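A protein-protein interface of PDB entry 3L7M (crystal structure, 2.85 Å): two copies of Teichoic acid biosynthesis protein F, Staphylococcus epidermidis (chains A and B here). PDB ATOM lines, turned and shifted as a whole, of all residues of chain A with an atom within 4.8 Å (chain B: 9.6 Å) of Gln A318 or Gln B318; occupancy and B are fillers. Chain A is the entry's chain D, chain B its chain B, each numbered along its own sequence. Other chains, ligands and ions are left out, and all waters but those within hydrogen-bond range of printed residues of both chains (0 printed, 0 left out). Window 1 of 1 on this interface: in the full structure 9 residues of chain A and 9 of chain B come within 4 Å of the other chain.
The backbone NH (N) of Lys B315 lies within hydrogen-bond range of the side-chain amide oxygen (OE1) of Gln A318 (2.8 Å).
The side-chain amide oxygen of Gln B318 lies within hydrogen-bond range of the backbone NH of Lys A315 (3.2 Å).
The side-chain amide nitrogen of Gln B318 sits close to the side-chain amide nitrogen of Gln A318 (3.2 Å).
Phe A314 touches Gln B318, and with the chains exchanged Gln A318 touches Phe B314.
Lys A315 touches Gln B318, and with the chains exchanged Gln A318 touches Lys B315.
Gln B318 touches its own counterpart, Gln A318.
Phe A319 touches Thr B322, and with the chains exchanged Thr A322 touches Phe B319.
Of the 15 pairs that touch across the chains among the printed residues, 12 have their exchanged pair printed and touching as well.
The side-chain hydroxyl (OG1) of Thr B322 sits at hydrogen-bond distance from the backbone carbonyl oxygen (O) of Gln B318, 3.3 Å away.
O of Gln A318 sits at hydrogen-bond distance from OG1 of Thr A322 (3.1 Å).
Printed residues of chain B that touch a printed residue of chain A: Ala B313, Phe B314, Lys B315, Gln B318, Phe B319, Thr B322, Leu B323 and Leu B343.
Hydrophobic or aromatic side chains of chain B within 4 Å of the printed part of chain A: Phe B314, Phe B319, Leu B323 and Leu B343.
Among the printed residues, 15 pairs touch across the chains.
Among the printed residues, no Asp or Glu carboxylate lies within 4 Å of a Lys or Arg side-chain nitrogen of the other chain.
Among the printed residues, pairs that only touch across the chains: Gln A318 with Phe B314, Thr A322 with Phe B319, Phe A314 with Gln B318, Phe A314 with Leu B343, Leu A343 with Phe B314, Phe A319 with Thr B322, Lys A315 with Ala B313, Thr A322 with Leu B323, Thr A322 with Thr B322, Phe A319 with Gln B318, Leu A343 with Phe B319 and Phe A319 with Leu B343.
Phe A314 touches two residues of chain B.
No residue of chain B comes within 4 Å of Asn A317.
Gln A318 touches just these residues of chain B: Phe B314, Lys B315 and Gln B318.
Printed residues of chain B within 4 Å of Phe A319: Gln B318 (3.9 Å), Thr B322 (3.6 Å) and Leu B343 (3.9 Å).
Of the printed residues of chain A, Ala B313 touches Lys A315.
Gln B318 touches four residues of chain A.
Printed residues of chain A within 4 Å of Thr B322: Phe A319 (3.6 Å) and Thr A322 (3.7 Å).
The nearest residue of chain B that does not touch Gln A318 is Phe B319 (4.1 Å).
The nearest printed residue of chain A that does not touch Gln B318 is Val A316 (5.3 Å).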
ATOM      1  N   PHE A 314     -22.854  10.829   8.597  1.00  0.00           N
ATOM      2  CA  PHE A 314     -23.771  10.343   9.626  1.00  0.00           C
ATOM      3  C   PHE A 314     -25.170  10.194   9.029  1.00  0.00           C
ATOM      4  O   PHE A 314     -25.676  11.113   8.400  1.00  0.00           O
ATOM      5  CB  PHE A 314     -23.793  11.304  10.821  1.00  0.00           C
ATOM      6  CG  PHE A 314     -24.539  10.780  12.031  1.00  0.00           C
ATOM      7  CD1 PHE A 314     -23.881  10.080  13.023  1.00  0.00           C
ATOM      8  CD2 PHE A 314     -25.898  11.005  12.185  1.00  0.00           C
ATOM      9  CE1 PHE A 314     -24.571   9.617  14.143  1.00  0.00           C
ATOM     10  CE2 PHE A 314     -26.590  10.534  13.304  1.00  0.00           C
ATOM     11  CZ  PHE A 314     -25.927   9.851  14.282  1.00  0.00           C
ATOM     12  N   LYS A 315     -25.788   9.033   9.200  1.00  0.00           N
ATOM     13  CA  LYS A 315     -27.126   8.835   8.673  1.00  0.00           C
ATOM     14  C   LYS A 315     -28.154   9.160   9.746  1.00  0.00           C
ATOM     15  O   LYS A 315     -28.469   8.324  10.582  1.00  0.00           O
ATOM     16  CB  LYS A 315     -27.309   7.412   8.140  1.00  0.00           C
ATOM     17  CG  LYS A 315     -26.862   7.246   6.689  1.00  0.00           C
ATOM     18  CD  LYS A 315     -27.164   5.848   6.161  1.00  0.00           C
ATOM     19  CE  LYS A 315     -28.666   5.615   5.897  1.00  0.00           C
ATOM     20  NZ  LYS A 315     -29.087   5.809   4.455  1.00  0.00           N
ATOM     21  N   VAL A 316     -28.682  10.380   9.716  1.00  0.00           N
ATOM     22  CA  VAL A 316     -29.558  10.850  10.788  1.00  0.00           C
ATOM     23  C   VAL A 316     -30.902  10.120  10.840  1.00  0.00           C
ATOM     24  O   VAL A 316     -31.481   9.990  11.903  1.00  0.00           O
ATOM     25  CB  VAL A 316     -29.699  12.413  10.811  1.00  0.00           C
ATOM     26  CG1 VAL A 316     -29.603  12.989   9.405  1.00  0.00           C
ATOM     27  CG2 VAL A 316     -30.983  12.858  11.515  1.00  0.00           C
ATOM     28  N   ASN A 317     -31.391   9.604   9.723  1.00  0.00           N
ATOM     29  CA  ASN A 317     -32.623   8.819   9.803  1.00  0.00           C
ATOM     30  C   ASN A 317     -32.434   7.468  10.476  1.00  0.00           C
ATOM     31  O   ASN A 317     -33.143   7.128  11.416  1.00  0.00           O
ATOM     32  CB  ASN A 317     -33.271   8.668   8.441  1.00  0.00           C
ATOM     33  CG  ASN A 317     -33.953   9.947   7.991  1.00  0.00           C
ATOM     34  OD1 ASN A 317     -34.644  10.603   8.782  1.00  0.00           O
ATOM     35  ND2 ASN A 317     -33.758  10.317   6.725  1.00  0.00           N
ATOM     36  N   GLN A 318     -31.463   6.701  10.003  1.00  0.00           N
ATOM     37  CA  GLN A 318     -31.115   5.434  10.642  1.00  0.00           C
ATOM     38  C   GLN A 318     -30.922   5.543  12.170  1.00  0.00           C
ATOM     39  O   GLN A 318     -31.246   4.609  12.915  1.00  0.00           O
ATOM     40  CB  GLN A 318     -29.854   4.874  10.009  1.00  0.00           C
ATOM     41  CG  GLN A 318     -29.701   3.406  10.205  1.00  0.00           C
ATOM     42  CD  GLN A 318     -28.281   2.969  10.042  1.00  0.00           C
ATOM     43  OE1 GLN A 318     -27.943   2.251   9.108  1.00  0.00           O
ATOM     44  NE2 GLN A 318     -27.431   3.405  10.952  1.00  0.00           N
ATOM     45  N   PHE A 319     -30.372   6.666  12.634  1.00  0.00           N
ATOM     46  CA  PHE A 319     -30.214   6.892  14.066  1.00  0.00           C
ATOM     47  C   PHE A 319     -31.606   6.934  14.709  1.00  0.00           C
ATOM     48  O   PHE A 319     -31.874   6.211  15.675  1.00  0.00           O
ATOM     49  CB  PHE A 319     -29.414   8.176  14.337  1.00  0.00           C
ATOM     50  CG  PHE A 319     -29.222   8.503  15.804  1.00  0.00           C
ATOM     51  CD1 PHE A 319     -28.322   7.802  16.578  1.00  0.00           C
ATOM     52  CD2 PHE A 319     -29.913   9.540  16.398  1.00  0.00           C
ATOM     53  CE1 PHE A 319     -28.127   8.113  17.919  1.00  0.00           C
ATOM     54  CE2 PHE A 319     -29.718   9.845  17.744  1.00  0.00           C
ATOM     55  CZ  PHE A 319     -28.821   9.129  18.495  1.00  0.00           C
ATOM     56  N   ARG A 320     -32.508   7.742  14.159  1.00  0.00           N
ATOM     57  CA  ARG A 320     -33.831   7.874  14.754  1.00  0.00           C
ATOM     58  C   ARG A 320     -34.581   6.542  14.868  1.00  0.00           C
ATOM     59  O   ARG A 320     -35.400   6.375  15.771  1.00  0.00           O
ATOM     60  CB  ARG A 320     -34.675   8.910  14.020  1.00  0.00           C
ATOM     61  CG  ARG A 320     -34.265  10.322  14.309  1.00  0.00           C
ATOM     62  CD  ARG A 320     -35.352  11.295  13.922  1.00  0.00           C
ATOM     63  NE  ARG A 320     -35.558  11.333  12.476  1.00  0.00           N
ATOM     64  CZ  ARG A 320     -36.393  12.167  11.855  1.00  0.00           C
ATOM     65  NH1 ARG A 320     -37.103  13.045  12.553  1.00  0.00           N
ATOM     66  NH2 ARG A 320     -36.513  12.125  10.533  1.00  0.00           N
ATOM     67  N   LYS A 321     -34.308   5.592  13.977  1.00  0.00           N
ATOM     68  CA  LYS A 321     -34.997   4.304  14.045  1.00  0.00           C
ATOM     69  C   LYS A 321     -34.348   3.332  15.035  1.00  0.00           C
ATOM     70  O   LYS A 321     -35.049   2.562  15.687  1.00  0.00           O
ATOM     71  CB  LYS A 321     -35.096   3.655  12.673  1.00  0.00           C
ATOM     72  CG  LYS A 321     -35.382   4.620  11.557  1.00  0.00           C
ATOM     73  CD  LYS A 321     -35.891   3.854  10.345  1.00  0.00           C
ATOM     74  CE  LYS A 321     -35.892   4.703   9.083  1.00  0.00           C
ATOM     75  NZ  LYS A 321     -35.796   3.833   7.875  1.00  0.00           N
ATOM     76  N   THR A 322     -33.018   3.354  15.143  1.00  0.00           N
ATOM     77  CA  THR A 322     -32.324   2.495  16.100  1.00  0.00           C
ATOM     78  C   THR A 322     -32.749   2.829  17.520  1.00  0.00           C
ATOM     79  O   THR A 322     -32.977   1.943  18.333  1.00  0.00           O
ATOM     80  CB  THR A 322     -30.813   2.664  16.025  1.00  0.00           C
ATOM     81  OG1 THR A 322     -30.361   2.287  14.726  1.00  0.00           O
ATOM     82  CG2 THR A 322     -30.145   1.780  17.053  1.00  0.00           C
ATOM     83  N   LEU A 343     -36.322  -0.446  10.630  1.00  0.00           N
ATOM     84  CA  LEU A 343     -34.869  -0.333  10.736  1.00  0.00           C
ATOM     85  C   LEU A 343     -34.218  -1.064   9.587  1.00  0.00           C
ATOM     86  O   LEU A 343     -33.280  -0.570   8.961  1.00  0.00           O
ATOM     87  CB  LEU A 343     -34.396  -1.027  12.008  1.00  0.00           C
ATOM     88  CG  LEU A 343     -33.453  -0.389  13.027  1.00  0.00           C
ATOM     89  CD1 LEU A 343     -32.703  -1.499  13.705  1.00  0.00           C
ATOM     90  CD2 LEU A 343     -32.497   0.611  12.415  1.00  0.00           C
ATOM     91  N   ALA B 313     -27.516   2.859   1.966  1.00  0.00           N
ATOM     92  CA  ALA B 313     -27.948   1.602   2.567  1.00  0.00           C
ATOM     93  C   ALA B 313     -27.568   1.600   4.030  1.00  0.00           C
ATOM     94  O   ALA B 313     -27.085   2.599   4.553  1.00  0.00           O
ATOM     95  CB  ALA B 313     -27.322   0.409   1.849  1.00  0.00           C
ATOM     96  N   PHE B 314     -27.776   0.469   4.686  1.00  0.00           N
ATOM     97  CA  PHE B 314     -27.585   0.405   6.122  1.00  0.00           C
ATOM     98  C   PHE B 314     -26.126   0.634   6.515  1.00  0.00           C
ATOM     99  O   PHE B 314     -25.248  -0.120   6.107  1.00  0.00           O
ATOM    100  CB  PHE B 314     -28.070  -0.939   6.652  1.00  0.00           C
ATOM    101  CG  PHE B 314     -28.338  -0.938   8.116  1.00  0.00           C
ATOM    102  CD1 PHE B 314     -29.595  -0.681   8.592  1.00  0.00           C
ATOM    103  CD2 PHE B 314     -27.331  -1.178   9.015  1.00  0.00           C
ATOM    104  CE1 PHE B 314     -29.846  -0.676   9.945  1.00  0.00           C
ATOM    105  CE2 PHE B 314     -27.576  -1.174  10.366  1.00  0.00           C
ATOM    106  CZ  PHE B 314     -28.834  -0.924  10.834  1.00  0.00           C
ATOM    107  N   LYS B 315     -25.874   1.677   7.307  1.00  0.00           N
ATOM    108  CA  LYS B 315     -24.533   1.973   7.806  1.00  0.00           C
ATOM    109  C   LYS B 315     -24.309   1.211   9.104  1.00  0.00           C
ATOM    110  O   LYS B 315     -24.722   1.653  10.180  1.00  0.00           O
ATOM    111  CB  LYS B 315     -24.353   3.478   8.028  1.00  0.00           C
ATOM    112  CG  LYS B 315     -22.919   3.973   7.902  1.00  0.00           C
ATOM    113  CD  LYS B 315     -22.815   5.474   8.185  1.00  0.00           C
ATOM    114  CE  LYS B 315     -21.358   5.970   8.201  1.00  0.00           C
ATOM    115  NZ  LYS B 315     -20.772   6.130   6.811  1.00  0.00           N
ATOM    116  N   VAL B 316     -23.648   0.061   8.990  1.00  0.00           N
ATOM    117  CA  VAL B 316     -23.535  -0.881  10.100  1.00  0.00           C
ATOM    118  C   VAL B 316     -22.560  -0.431  11.187  1.00  0.00           C
ATOM    119  O   VAL B 316     -22.837  -0.607  12.373  1.00  0.00           O
ATOM    120  CB  VAL B 316     -23.280  -2.357   9.612  1.00  0.00           C
ATOM    121  CG1 VAL B 316     -22.523  -2.383   8.289  1.00  0.00           C
ATOM    122  CG2 VAL B 316     -22.571  -3.177  10.678  1.00  0.00           C
ATOM    123  N   ASN B 317     -21.435   0.164  10.804  1.00  0.00           N
ATOM    124  CA  ASN B 317     -20.517   0.686  11.814  1.00  0.00           C
ATOM    125  C   ASN B 317     -21.214   1.676  12.758  1.00  0.00           C
ATOM    126  O   ASN B 317     -21.128   1.555  13.974  1.00  0.00           O
ATOM    127  CB  ASN B 317     -19.260   1.283  11.175  1.00  0.00           C
ATOM    128  CG  ASN B 317     -18.159   0.224  10.934  1.00  0.00           C
ATOM    129  OD1 ASN B 317     -18.449  -0.957  10.743  1.00  0.00           O
ATOM    130  ND2 ASN B 317     -16.891   0.660  10.943  1.00  0.00           N
ATOM    131  N   GLN B 318     -21.939   2.631  12.199  1.00  0.00           N
ATOM    132  CA  GLN B 318     -22.757   3.526  13.014  1.00  0.00           C
ATOM    133  C   GLN B 318     -23.738   2.800  13.933  1.00  0.00           C
ATOM    134  O   GLN B 318     -23.851   3.129  15.122  1.00  0.00           O
ATOM    135  CB  GLN B 318     -23.537   4.499  12.150  1.00  0.00           C
ATOM    136  CG  GLN B 318     -24.504   5.295  12.960  1.00  0.00           C
ATOM    137  CD  GLN B 318     -25.245   6.300  12.128  1.00  0.00           C
ATOM    138  OE1 GLN B 318     -24.647   7.157  11.479  1.00  0.00           O
ATOM    139  NE2 GLN B 318     -26.561   6.203  12.137  1.00  0.00           N
ATOM    140  N   PHE B 319     -24.473   1.838  13.389  1.00  0.00           N
ATOM    141  CA  PHE B 319     -25.411   1.088  14.211  1.00  0.00           C
ATOM    142  C   PHE B 319     -24.691   0.527  15.418  1.00  0.00           C
ATOM    143  O   PHE B 319     -25.190   0.636  16.535  1.00  0.00           O
ATOM    144  CB  PHE B 319     -26.045  -0.046  13.425  1.00  0.00           C
ATOM    145  CG  PHE B 319     -27.022  -0.853  14.210  1.00  0.00           C
ATOM    146  CD1 PHE B 319     -28.243  -0.325  14.567  1.00  0.00           C
ATOM    147  CD2 PHE B 319     -26.734  -2.155  14.561  1.00  0.00           C
ATOM    148  CE1 PHE B 319     -29.157  -1.080  15.279  1.00  0.00           C
ATOM    149  CE2 PHE B 319     -27.643  -2.912  15.271  1.00  0.00           C
ATOM    150  CZ  PHE B 319     -28.853  -2.373  15.631  1.00  0.00           C
ATOM    151  N   ARG B 320     -23.512  -0.053  15.206  1.00  0.00           N
ATOM    152  CA  ARG B 320     -22.781  -0.674  16.303  1.00  0.00           C
ATOM    153  C   ARG B 320     -22.493   0.311  17.420  1.00  0.00           C
ATOM    154  O   ARG B 320     -22.626  -0.030  18.587  1.00  0.00           O
ATOM    155  CB  ARG B 320     -21.486  -1.324  15.814  1.00  0.00           C
ATOM    156  CG  ARG B 320     -21.683  -2.691  15.173  1.00  0.00           C
ATOM    157  CD  ARG B 320     -20.406  -3.492  15.212  1.00  0.00           C
ATOM    158  NE  ARG B 320     -19.498  -3.141  14.121  1.00  0.00           N
ATOM    159  CZ  ARG B 320     -18.181  -3.363  14.131  1.00  0.00           C
ATOM    160  NH1 ARG B 320     -17.599  -3.923  15.188  1.00  0.00           N
ATOM    161  NH2 ARG B 320     -17.441  -3.013  13.084  1.00  0.00           N
ATOM    162  N   LYS B 321     -22.103   1.530  17.057  1.00  0.00           N
ATOM    163  CA  LYS B 321     -21.836   2.581  18.034  1.00  0.00           C
ATOM    164  C   LYS B 321     -23.102   3.074  18.735  1.00  0.00           C
ATOM    165  O   LYS B 321     -23.101   3.275  19.951  1.00  0.00           O
ATOM    166  CB  LYS B 321     -21.141   3.762  17.379  1.00  0.00           C
ATOM    167  CG  LYS B 321     -20.056   3.373  16.417  1.00  0.00           C
ATOM    168  CD  LYS B 321     -19.163   4.561  16.093  1.00  0.00           C
ATOM    169  CE  LYS B 321     -18.089   4.189  15.074  1.00  0.00           C
ATOM    170  NZ  LYS B 321     -17.148   5.326  14.816  1.00  0.00           N
ATOM    171  N   THR B 322     -24.182   3.286  17.990  1.00  0.00           N
ATOM    172  CA  THR B 322     -25.424   3.714  18.631  1.00  0.00           C
ATOM    173  C   THR B 322     -25.881   2.738  19.721  1.00  0.00           C
ATOM    174  O   THR B 322     -26.355   3.151  20.783  1.00  0.00           O
ATOM    175  CB  THR B 322     -26.560   3.901  17.624  1.00  0.00           C
ATOM    176  OG1 THR B 322     -26.176   4.888  16.665  1.00  0.00           O
ATOM    177  CG2 THR B 322     -27.812   4.369  18.334  1.00  0.00           C
ATOM    178  N   LEU B 323     -25.743   1.443  19.452  1.00  0.00           N
ATOM    179  CA  LEU B 323     -26.083   0.426  20.441  1.00  0.00           C
ATOM    180  C   LEU B 323     -25.136   0.500  21.632  1.00  0.00           C
ATOM    181  O   LEU B 323     -25.553   0.411  22.780  1.00  0.00           O
ATOM    182  CB  LEU B 323     -26.037  -0.968  19.820  1.00  0.00           C
ATOM    183  CG  LEU B 323     -27.388  -1.658  19.642  1.00  0.00           C
ATOM    184  CD1 LEU B 323     -28.481  -0.673  19.287  1.00  0.00           C
ATOM    185  CD2 LEU B 323     -27.284  -2.748  18.598  1.00  0.00           C
ATOM    186  N   ARG B 324     -23.851   0.662  21.352  1.00  0.00           N
ATOM    187  CA  ARG B 324     -22.860   0.692  22.409  1.00  0.00           C
ATOM    188  C   ARG B 324     -23.179   1.856  23.325  1.00  0.00           C
ATOM    189  O   ARG B 324     -23.228   1.709  24.547  1.00  0.00           O
ATOM    190  CB  ARG B 324     -21.475   0.847  21.803  1.00  0.00           C
ATOM    191  CG  ARG B 324     -20.354   0.342  22.660  1.00  0.00           C
ATOM    192  CD  ARG B 324     -19.376  -0.442  21.793  1.00  0.00           C
ATOM    193  NE  ARG B 324     -18.824   0.320  20.664  1.00  0.00           N
ATOM    194  CZ  ARG B 324     -18.459  -0.219  19.496  1.00  0.00           C
ATOM    195  NH1 ARG B 324     -18.615  -1.527  19.281  1.00  0.00           N
ATOM    196  NH2 ARG B 324     -17.948   0.546  18.529  1.00  0.00           N
ATOM    197  N   HIS B 325     -23.428   3.014  22.720  1.00  0.00           N
ATOM    198  CA  HIS B 325     -23.682   4.230  23.481  1.00  0.00           C
ATOM    199  C   HIS B 325     -24.985   4.137  24.274  1.00  0.00           C
ATOM    200  O   HIS B 325     -25.030   4.452  25.465  1.00  0.00           O
ATOM    201  CB  HIS B 325     -23.717   5.437  22.567  1.00  0.00           C
ATOM    202  CG  HIS B 325     -23.902   6.716  23.306  1.00  0.00           C
ATOM    203  ND1 HIS B 325     -22.938   7.230  24.144  1.00  0.00           N
ATOM    204  CD2 HIS B 325     -24.948   7.575  23.363  1.00  0.00           C
ATOM    205  CE1 HIS B 325     -23.375   8.355  24.678  1.00  0.00           C
ATOM    206  NE2 HIS B 325     -24.592   8.591  24.215  1.00  0.00           N
ATOM    207  N   VAL B 326     -26.052   3.696  23.614  1.00  0.00           N
ATOM    208  CA  VAL B 326     -27.280   3.410  24.338  1.00  0.00           C
ATOM    209  C   VAL B 326     -26.978   2.539  25.556  1.00  0.00           C
ATOM    210  O   VAL B 326     -27.553   2.734  26.620  1.00  0.00           O
ATOM    211  CB  VAL B 326     -28.297   2.714  23.459  1.00  0.00           C
ATOM    212  CG1 VAL B 326     -29.401   2.142  24.318  1.00  0.00           C
ATOM    213  CG2 VAL B 326     -28.846   3.694  22.445  1.00  0.00           C
ATOM    214  N   SER B 339     -18.178   6.856  24.408  1.00  0.00           N
ATOM    215  CA  SER B 339     -18.994   6.314  23.322  1.00  0.00           C
ATOM    216  C   SER B 339     -19.817   7.373  22.588  1.00  0.00           C
ATOM    217  O   SER B 339     -20.065   7.238  21.390  1.00  0.00           O
ATOM    218  CB  SER B 339     -19.898   5.200  23.821  1.00  0.00           C
ATOM    219  OG  SER B 339     -20.732   5.655  24.859  1.00  0.00           O
ATOM    220  N   ASP B 342     -17.276   8.703  20.118  1.00  0.00           N
ATOM    221  CA  ASP B 342     -17.069   7.787  18.998  1.00  0.00           C
ATOM    222  C   ASP B 342     -18.189   7.890  17.931  1.00  0.00           C
ATOM    223  O   ASP B 342     -17.941   7.766  16.727  1.00  0.00           O
ATOM    224  CB  ASP B 342     -16.942   6.362  19.551  1.00  0.00           C
ATOM    225  CG  ASP B 342     -16.362   5.386  18.545  1.00  0.00           C
ATOM    226  OD1 ASP B 342     -15.588   5.832  17.651  1.00  0.00           O
ATOM    227  OD2 ASP B 342     -16.692   4.175  18.661  1.00  0.00           O
ATOM    228  N   LEU B 343     -19.408   8.148  18.394  1.00  0.00           N
ATOM    229  CA  LEU B 343     -20.601   8.157  17.557  1.00  0.00           C
ATOM    230  C   LEU B 343     -20.639   9.427  16.732  1.00  0.00           C
ATOM    231  O   LEU B 343     -21.072   9.437  15.572  1.00  0.00           O
ATOM    232  CB  LEU B 343     -21.837   8.131  18.455  1.00  0.00           C
ATOM    233  CG  LEU B 343     -23.076   7.367  18.006  1.00  0.00           C
ATOM    234  CD1 LEU B 343     -24.287   7.856  18.776  1.00  0.00           C
ATOM    235  CD2 LEU B 343     -23.290   7.566  16.546  1.00  0.00           C
ATOM    236  N   THR B 344     -20.178  10.512  17.340  1.00  0.00           N
ATOM    237  CA  THR B 344     -20.379  11.822  16.755  1.00  0.00           C
ATOM    238  C   THR B 344     -19.125  12.439  16.135  1.00  0.00           C
ATOM    239  O   THR B 344     -19.231  13.242  15.207  1.00  0.00           O
ATOM    240  CB  THR B 344     -20.972  12.775  17.784  1.00  0.00           C
ATOM    241  OG1 THR B 344     -19.939  13.246  18.657  1.00  0.00           O
ATOM    242  CG2 THR B 344     -22.032  12.052  18.589  1.00  0.00           C
ATOM    243  N   ASP B 345     -17.948  12.068  16.636  1.00  0.00           N
ATOM    244  CA  ASP B 345     -16.691  12.506  16.038  1.00  0.00           C
ATOM    245  C   ASP B 345     -16.747  12.416  14.523  1.00  0.00           C
ATOM    246  O   ASP B 345     -17.065  11.371  13.961  1.00  0.00           O
ATOM    247  CB  ASP B 345     -15.526  11.661  16.544  1.00  0.00           C
ATOM    248  CG  ASP B 345     -14.191  12.088  15.951  1.00  0.00           C
ATOM    249  OD1 ASP B 345     -14.018  13.293  15.667  1.00  0.00           O
ATOM    250  OD2 ASP B 345     -13.314  11.216  15.765  1.00  0.00           O
